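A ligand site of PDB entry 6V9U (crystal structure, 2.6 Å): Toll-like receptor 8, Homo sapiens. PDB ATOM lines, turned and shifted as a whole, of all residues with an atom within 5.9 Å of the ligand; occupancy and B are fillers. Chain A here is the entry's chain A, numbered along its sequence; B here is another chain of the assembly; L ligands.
N of Gly 329 sits at hydrogen-bond distance from O1 of the ligand, at 2.8 Å. The backbone carbonyl oxygen (O) of Phe 472 of chain B sits at hydrogen-bond distance from a nitrogen (N2) of the ligand (2.7 Å). N1 of the ligand lies within salt-bridge range of OE1 of Glu 405, 2.9 Å away.
OH of Tyr 331 lies within hydrogen-bond range of O of Phe 383 (2.7 Å). The backbone carbonyl oxygen (O) of Phe 472 of chain B is in hydrogen-bond range of the backbone NH (N) of Ala 496 of chain B (3.0 Å). N of Ile 474 of chain B is in hydrogen-bond range of OE1 of Gln 497 of chain B. The backbone NH (N) of Tyr 326 sits close to the backbone carbonyl oxygen (O) of Gly 354.
Merely in contact with the ligand: Phe 239, Tyr 326, Ile 327, Lys 328, Ser 330, Val 356, Phe 383, Phe 473 of chain B, Ser 494 of chain B, Ala 496 of chain B and Gln 497 of chain B. Of the 22 residues printed, 14 come within 4 Å of the ligand. The nearest printed residue that does not touch the ligand is Ile 381 (4.01 Å).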
ATOM      1  N   PHE A 239       5.472 -18.451 -21.239  1.00  0.00           N
ATOM      2  CA  PHE A 239       4.335 -17.560 -21.002  1.00  0.00           C
ATOM      3  C   PHE A 239       3.503 -18.042 -19.791  1.00  0.00           C
ATOM      4  O   PHE A 239       4.010 -18.783 -18.951  1.00  0.00           O
ATOM      5  CB  PHE A 239       3.470 -17.516 -22.274  1.00  0.00           C
ATOM      6  CG  PHE A 239       3.207 -16.135 -22.805  1.00  0.00           C
ATOM      7  CD1 PHE A 239       4.120 -15.524 -23.653  1.00  0.00           C
ATOM      8  CD2 PHE A 239       2.037 -15.460 -22.483  1.00  0.00           C
ATOM      9  CE1 PHE A 239       3.873 -14.244 -24.154  1.00  0.00           C
ATOM     10  CE2 PHE A 239       1.789 -14.180 -22.984  1.00  0.00           C
ATOM     11  CZ  PHE A 239       2.717 -13.573 -23.816  1.00  0.00           C
ATOM     12  N   PHE A 324       0.866 -13.433 -30.122  1.00  0.00           N
ATOM     13  CA  PHE A 324       2.017 -13.190 -29.246  1.00  0.00           C
ATOM     14  C   PHE A 324       3.370 -13.467 -29.937  1.00  0.00           C
ATOM     15  O   PHE A 324       4.166 -14.310 -29.485  1.00  0.00           O
ATOM     16  CB  PHE A 324       1.857 -13.957 -27.907  1.00  0.00           C
ATOM     17  CG  PHE A 324       0.634 -13.538 -27.123  1.00  0.00           C
ATOM     18  CD1 PHE A 324       0.659 -12.431 -26.299  1.00  0.00           C
ATOM     19  CD2 PHE A 324      -0.550 -14.268 -27.219  1.00  0.00           C
ATOM     20  CE1 PHE A 324      -0.488 -12.042 -25.572  1.00  0.00           C
ATOM     21  CE2 PHE A 324      -1.693 -13.876 -26.501  1.00  0.00           C
ATOM     22  CZ  PHE A 324      -1.645 -12.776 -25.680  1.00  0.00           C
ATOM     23  N   TYR A 326       5.331 -10.656 -30.817  1.00  0.00           N
ATOM     24  CA  TYR A 326       6.005  -9.389 -30.489  1.00  0.00           C
ATOM     25  C   TYR A 326       7.488  -9.490 -30.154  1.00  0.00           C
ATOM     26  O   TYR A 326       7.945 -10.493 -29.607  1.00  0.00           O
ATOM     27  CB  TYR A 326       5.266  -8.675 -29.330  1.00  0.00           C
ATOM     28  CG  TYR A 326       5.424  -9.320 -27.960  1.00  0.00           C
ATOM     29  CD1 TYR A 326       4.619 -10.383 -27.569  1.00  0.00           C
ATOM     30  CD2 TYR A 326       6.364  -8.842 -27.051  1.00  0.00           C
ATOM     31  CE1 TYR A 326       4.753 -10.974 -26.318  1.00  0.00           C
ATOM     32  CE2 TYR A 326       6.516  -9.424 -25.789  1.00  0.00           C
ATOM     33  CZ  TYR A 326       5.701 -10.490 -25.426  1.00  0.00           C
ATOM     34  OH  TYR A 326       5.851 -11.066 -24.185  1.00  0.00           O
ATOM     35  N   ILE A 327       8.233  -8.408 -30.450  1.00  0.00           N
ATOM     36  CA  ILE A 327       9.647  -8.266 -30.109  1.00  0.00           C
ATOM     37  C   ILE A 327       9.672  -7.622 -28.710  1.00  0.00           C
ATOM     38  O   ILE A 327       8.966  -6.639 -28.483  1.00  0.00           O
ATOM     39  CB  ILE A 327      10.437  -7.417 -31.159  1.00  0.00           C
ATOM     40  CG1 ILE A 327      10.268  -7.978 -32.593  1.00  0.00           C
ATOM     41  CG2 ILE A 327      11.932  -7.290 -30.776  1.00  0.00           C
ATOM     42  CD1 ILE A 327      10.626  -6.990 -33.738  1.00  0.00           C
ATOM     43  N   LYS A 328      10.452  -8.210 -27.781  1.00  0.00           N
ATOM     44  CA  LYS A 328      10.604  -7.762 -26.392  1.00  0.00           C
ATOM     45  C   LYS A 328      11.117  -6.313 -26.336  1.00  0.00           C
ATOM     46  O   LYS A 328      12.162  -6.003 -26.908  1.00  0.00           O
ATOM     47  CB  LYS A 328      11.537  -8.706 -25.630  1.00  0.00           C
ATOM     48  CG  LYS A 328      11.357  -8.680 -24.114  1.00  0.00           C
ATOM     49  CD  LYS A 328      12.308  -9.650 -23.399  1.00  0.00           C
ATOM     50  CE  LYS A 328      13.536  -8.969 -22.845  1.00  0.00           C
ATOM     51  NZ  LYS A 328      14.380  -9.912 -22.076  1.00  0.00           N
ATOM     52  N   GLY A 329      10.341  -5.456 -25.669  1.00  0.00           N
ATOM     53  CA  GLY A 329      10.651  -4.038 -25.494  1.00  0.00           C
ATOM     54  C   GLY A 329      10.326  -3.159 -26.676  1.00  0.00           C
ATOM     55  O   GLY A 329      10.637  -1.957 -26.653  1.00  0.00           O
ATOM     56  N   SER A 330       9.699  -3.728 -27.719  1.00  0.00           N
ATOM     57  CA  SER A 330       9.342  -3.007 -28.944  1.00  0.00           C
ATOM     58  C   SER A 330       7.838  -2.710 -29.029  1.00  0.00           C
ATOM     59  O   SER A 330       7.021  -3.642 -29.010  1.00  0.00           O
ATOM     60  CB  SER A 330       9.817  -3.763 -30.175  1.00  0.00           C
ATOM     61  OG  SER A 330       9.742  -2.952 -31.339  1.00  0.00           O
ATOM     62  N   TYR A 331       7.496  -1.423 -29.124  1.00  0.00           N
ATOM     63  CA  TYR A 331       6.134  -0.913 -29.214  1.00  0.00           C
ATOM     64  C   TYR A 331       5.998  -0.098 -30.517  1.00  0.00           C
ATOM     65  O   TYR A 331       6.019   1.136 -30.473  1.00  0.00           O
ATOM     66  CB  TYR A 331       5.816  -0.056 -27.961  1.00  0.00           C
ATOM     67  CG  TYR A 331       4.368   0.292 -27.709  1.00  0.00           C
ATOM     68  CD1 TYR A 331       3.336  -0.518 -28.198  1.00  0.00           C
ATOM     69  CD2 TYR A 331       4.018   1.362 -26.900  1.00  0.00           C
ATOM     70  CE1 TYR A 331       2.001  -0.225 -27.938  1.00  0.00           C
ATOM     71  CE2 TYR A 331       2.688   1.661 -26.624  1.00  0.00           C
ATOM     72  CZ  TYR A 331       1.680   0.862 -27.145  1.00  0.00           C
ATOM     73  OH  TYR A 331       0.373   1.163 -26.871  1.00  0.00           O
ATOM     74  N   GLY A 354      -1.319 -10.171 -29.355  1.00  0.00           N
ATOM     75  CA  GLY A 354       0.024  -9.913 -28.857  1.00  0.00           C
ATOM     76  C   GLY A 354       1.112  -9.501 -29.832  1.00  0.00           C
ATOM     77  O   GLY A 354       2.264  -9.870 -29.639  1.00  0.00           O
ATOM     78  N   VAL A 356       1.542  -6.264 -30.356  1.00  0.00           N
ATOM     79  CA  VAL A 356       1.838  -5.058 -29.575  1.00  0.00           C
ATOM     80  C   VAL A 356       2.184  -3.891 -30.518  1.00  0.00           C
ATOM     81  O   VAL A 356       3.326  -3.762 -30.949  1.00  0.00           O
ATOM     82  CB  VAL A 356       2.896  -5.264 -28.444  1.00  0.00           C
ATOM     83  CG1 VAL A 356       2.957  -4.060 -27.515  1.00  0.00           C
ATOM     84  CG2 VAL A 356       2.613  -6.533 -27.634  1.00  0.00           C
ATOM     85  N   ILE A 381      -5.364  -7.926 -26.918  1.00  0.00           N
ATOM     86  CA  ILE A 381      -4.081  -7.737 -26.207  1.00  0.00           C
ATOM     87  C   ILE A 381      -2.989  -7.221 -27.180  1.00  0.00           C
ATOM     88  O   ILE A 381      -1.990  -7.900 -27.429  1.00  0.00           O
ATOM     89  CB  ILE A 381      -3.645  -9.003 -25.380  1.00  0.00           C
ATOM     90  CG1 ILE A 381      -4.834  -9.628 -24.599  1.00  0.00           C
ATOM     91  CG2 ILE A 381      -2.480  -8.677 -24.425  1.00  0.00           C
ATOM     92  CD1 ILE A 381      -4.779 -11.139 -24.464  1.00  0.00           C
ATOM     93  N   PHE A 383      -2.648  -3.510 -27.242  1.00  0.00           N
ATOM     94  CA  PHE A 383      -2.502  -2.183 -26.634  1.00  0.00           C
ATOM     95  C   PHE A 383      -2.629  -1.049 -27.667  1.00  0.00           C
ATOM     96  O   PHE A 383      -1.908  -0.051 -27.580  1.00  0.00           O
ATOM     97  CB  PHE A 383      -1.198  -2.101 -25.802  1.00  0.00           C
ATOM     98  CG  PHE A 383      -1.073  -3.130 -24.700  1.00  0.00           C
ATOM     99  CD1 PHE A 383      -1.604  -2.890 -23.437  1.00  0.00           C
ATOM    100  CD2 PHE A 383      -0.417  -4.335 -24.932  1.00  0.00           C
ATOM    101  CE1 PHE A 383      -1.482  -3.840 -22.425  1.00  0.00           C
ATOM    102  CE2 PHE A 383      -0.299  -5.288 -23.911  1.00  0.00           C
ATOM    103  CZ  PHE A 383      -0.833  -5.033 -22.666  1.00  0.00           C
ATOM    104  N   GLU A 405      -9.157  -5.805 -24.629  1.00  0.00           N
ATOM    105  CA  GLU A 405      -7.877  -5.628 -23.912  1.00  0.00           C
ATOM    106  C   GLU A 405      -6.879  -4.755 -24.704  1.00  0.00           C
ATOM    107  O   GLU A 405      -5.692  -5.077 -24.799  1.00  0.00           O
ATOM    108  CB  GLU A 405      -7.275  -6.978 -23.463  1.00  0.00           C
ATOM    109  CG  GLU A 405      -7.987  -7.592 -22.267  1.00  0.00           C
ATOM    110  CD  GLU A 405      -7.750  -9.082 -22.046  1.00  0.00           C
ATOM    111  OE1 GLU A 405      -7.470  -9.465 -20.889  1.00  0.00           O
ATOM    112  OE2 GLU A 405      -7.883  -9.850 -23.020  1.00  0.00           O
ATOM    113  N   PHE B 472       2.555  -0.964 -19.169  1.00  0.00           N
ATOM    114  CA  PHE B 472       2.478  -2.429 -19.155  1.00  0.00           C
ATOM    115  C   PHE B 472       3.863  -3.103 -19.212  1.00  0.00           C
ATOM    116  O   PHE B 472       3.968  -4.328 -19.039  1.00  0.00           O
ATOM    117  CB  PHE B 472       1.517  -2.965 -20.228  1.00  0.00           C
ATOM    118  CG  PHE B 472       1.843  -2.656 -21.671  1.00  0.00           C
ATOM    119  CD1 PHE B 472       1.394  -1.479 -22.271  1.00  0.00           C
ATOM    120  CD2 PHE B 472       2.538  -3.567 -22.460  1.00  0.00           C
ATOM    121  CE1 PHE B 472       1.656  -1.213 -23.619  1.00  0.00           C
ATOM    122  CE2 PHE B 472       2.800  -3.301 -23.808  1.00  0.00           C
ATOM    123  CZ  PHE B 472       2.371  -2.122 -24.376  1.00  0.00           C
ATOM    124  N   PHE B 473       4.917  -2.293 -19.420  1.00  0.00           N
ATOM    125  CA  PHE B 473       6.342  -2.648 -19.410  1.00  0.00           C
ATOM    126  C   PHE B 473       7.145  -1.347 -19.335  1.00  0.00           C
ATOM    127  O   PHE B 473       6.694  -0.324 -19.839  1.00  0.00           O
ATOM    128  CB  PHE B 473       6.758  -3.521 -20.615  1.00  0.00           C
ATOM    129  CG  PHE B 473       7.084  -2.834 -21.920  1.00  0.00           C
ATOM    130  CD1 PHE B 473       8.390  -2.423 -22.197  1.00  0.00           C
ATOM    131  CD2 PHE B 473       6.114  -2.675 -22.903  1.00  0.00           C
ATOM    132  CE1 PHE B 473       8.686  -1.797 -23.410  1.00  0.00           C
ATOM    133  CE2 PHE B 473       6.433  -2.057 -24.120  1.00  0.00           C
ATOM    134  CZ  PHE B 473       7.716  -1.625 -24.366  1.00  0.00           C
ATOM    135  N   ILE B 474       8.326  -1.379 -18.686  1.00  0.00           N
ATOM    136  CA  ILE B 474       9.164  -0.190 -18.575  1.00  0.00           C
ATOM    137  C   ILE B 474       9.991  -0.012 -19.856  1.00  0.00           C
ATOM    138  O   ILE B 474      10.915  -0.800 -20.117  1.00  0.00           O
ATOM    139  CB  ILE B 474      10.005  -0.154 -17.264  1.00  0.00           C
ATOM    140  CG1 ILE B 474       9.098  -0.223 -16.017  1.00  0.00           C
ATOM    141  CG2 ILE B 474      10.902   1.089 -17.213  1.00  0.00           C
ATOM    142  CD1 ILE B 474       9.445  -1.346 -15.066  1.00  0.00           C
ATOM    143  N   SER B 494      -0.234  -2.943 -14.141  1.00  0.00           N
ATOM    144  CA  SER B 494      -0.310  -4.264 -14.786  1.00  0.00           C
ATOM    145  C   SER B 494       1.030  -4.596 -15.478  1.00  0.00           C
ATOM    146  O   SER B 494       1.046  -5.392 -16.421  1.00  0.00           O
ATOM    147  CB  SER B 494      -1.490  -4.346 -15.758  1.00  0.00           C
ATOM    148  OG  SER B 494      -2.709  -3.933 -15.168  1.00  0.00           O
ATOM    149  N   ASN B 495       2.135  -4.014 -14.976  1.00  0.00           N
ATOM    150  CA  ASN B 495       3.499  -4.142 -15.499  1.00  0.00           C
ATOM    151  C   ASN B 495       4.011  -5.586 -15.462  1.00  0.00           C
ATOM    152  O   ASN B 495       4.099  -6.161 -14.385  1.00  0.00           O
ATOM    153  CB  ASN B 495       4.435  -3.218 -14.717  1.00  0.00           C
ATOM    154  CG  ASN B 495       5.530  -2.612 -15.533  1.00  0.00           C
ATOM    155  OD1 ASN B 495       6.419  -3.298 -16.038  1.00  0.00           O
ATOM    156  ND2 ASN B 495       5.514  -1.302 -15.650  1.00  0.00           N
ATOM    157  N   ALA B 496       4.358  -6.152 -16.629  1.00  0.00           N
ATOM    158  CA  ALA B 496       4.858  -7.524 -16.767  1.00  0.00           C
ATOM    159  C   ALA B 496       6.322  -7.600 -17.263  1.00  0.00           C
ATOM    160  O   ALA B 496       6.748  -8.626 -17.809  1.00  0.00           O
ATOM    161  CB  ALA B 496       3.932  -8.329 -17.665  1.00  0.00           C
ATOM    162  N   GLN B 497       7.091  -6.521 -17.049  1.00  0.00           N
ATOM    163  CA  GLN B 497       8.498  -6.371 -17.438  1.00  0.00           C
ATOM    164  C   GLN B 497       9.412  -7.404 -16.770  1.00  0.00           C
ATOM    165  O   GLN B 497       9.307  -7.636 -15.560  1.00  0.00           O
ATOM    166  CB  GLN B 497       8.976  -4.940 -17.118  1.00  0.00           C
ATOM    167  CG  GLN B 497      10.451  -4.622 -17.421  1.00  0.00           C
ATOM    168  CD  GLN B 497      10.736  -4.314 -18.871  1.00  0.00           C
ATOM    169  OE1 GLN B 497       9.990  -3.584 -19.531  1.00  0.00           O
ATOM    170  NE2 GLN B 497      11.854  -4.808 -19.360  1.00  0.00           N
ATOM    171  N   VAL B 498      10.316  -8.004 -17.559  1.00  0.00           N
ATOM    172  CA  VAL B 498      11.340  -8.926 -17.092  1.00  0.00           C
ATOM    173  C   VAL B 498      12.520  -7.995 -16.760  1.00  0.00           C
ATOM    174  O   VAL B 498      13.252  -7.582 -17.661  1.00  0.00           O
ATOM    175  CB  VAL B 498      11.700 -10.021 -18.133  1.00  0.00           C
ATOM    176  CG1 VAL B 498      12.803 -10.939 -17.619  1.00  0.00           C
ATOM    177  CG2 VAL B 498      10.471 -10.846 -18.519  1.00  0.00           C
ATOM    178  N   ARG B 519       2.630  -7.485 -12.386  1.00  0.00           N
ATOM    179  CA  ARG B 519       2.863  -8.835 -12.917  1.00  0.00           C
ATOM    180  C   ARG B 519       4.362  -9.009 -13.249  1.00  0.00           C
ATOM    181  O   ARG B 519       4.711  -9.851 -14.085  1.00  0.00           O
ATOM    182  CB  ARG B 519       2.039  -9.034 -14.207  1.00  0.00           C
ATOM    183  CG  ARG B 519       0.529  -8.893 -14.085  1.00  0.00           C
ATOM    184  CD  ARG B 519      -0.117  -8.831 -15.462  1.00  0.00           C
ATOM    185  NE  ARG B 519      -1.507  -9.281 -15.428  1.00  0.00           N
ATOM    186  CZ  ARG B 519      -1.915 -10.488 -15.813  1.00  0.00           C
ATOM    187  NH1 ARG B 519      -1.041 -11.376 -16.277  1.00  0.00           N
ATOM    188  NH2 ARG B 519      -3.198 -10.817 -15.738  1.00  0.00           N
HETATM  189  N1  LIG L   1      -4.566  -9.655 -20.560  1.00  0.00           N
HETATM  190  C1  LIG L   1       1.541  -7.708 -21.344  1.00  0.00           C
HETATM  191  C2  LIG L   1       0.241  -8.225 -21.271  1.00  0.00           C
HETATM  192  C3  LIG L   1       3.709  -7.152 -21.723  1.00  0.00           C
HETATM  193  C4  LIG L   1       2.656  -7.894 -22.234  1.00  0.00           C
HETATM  194  C5  LIG L   1       2.674  -8.703 -23.521  1.00  0.00           C
HETATM  195  C6  LIG L   1       1.723  -8.169 -24.564  1.00  0.00           C
HETATM  196  C7  LIG L   1       5.398  -6.513 -23.434  1.00  0.00           C
HETATM  197  C8  LIG L   1       7.742  -6.385 -22.853  1.00  0.00           C
HETATM  198  C9  LIG L   1       6.154  -7.175 -21.241  1.00  0.00           C
HETATM  199  C10 LIG L   1      -3.449 -10.489 -20.046  1.00  0.00           C
HETATM  200  C11 LIG L   1      -4.433  -8.239 -20.144  1.00  0.00           C
HETATM  201  C12 LIG L   1      -3.112  -7.659 -20.598  1.00  0.00           C
HETATM  202  C13 LIG L   1      10.043  -5.964 -22.320  1.00  0.00           C
HETATM  203  O1  LIG L   1       8.988  -5.978 -23.272  1.00  0.00           O
HETATM  204  C14 LIG L   1       6.711  -6.223 -23.793  1.00  0.00           C
HETATM  205  O2  LIG L   1       7.097  -5.791 -25.032  1.00  0.00           O
HETATM  206  C15 LIG L   1       6.086  -5.469 -25.979  1.00  0.00           C
HETATM  207  C16 LIG L   1       7.458  -6.871 -21.577  1.00  0.00           C
HETATM  208  C17 LIG L   1       5.112  -6.980 -22.152  1.00  0.00           C
HETATM  209  N2  LIG L   1       3.286  -6.503 -20.573  1.00  0.00           N
HETATM  210  C18 LIG L   1       1.966  -6.832 -20.332  1.00  0.00           C
HETATM  211  C19 LIG L   1       1.135  -6.445 -19.298  1.00  0.00           C
HETATM  212  C20 LIG L   1      -0.130  -6.999 -19.233  1.00  0.00           C
HETATM  213  C21 LIG L   1       2.470 -10.183 -23.282  1.00  0.00           C
HETATM  214  C22 LIG L   1      -0.596  -7.891 -20.200  1.00  0.00           C
HETATM  215  C23 LIG L   1      -1.973  -8.506 -20.033  1.00  0.00           C
HETATM  216  C24 LIG L   1      -2.121  -9.944 -20.519  1.00  0.00           C
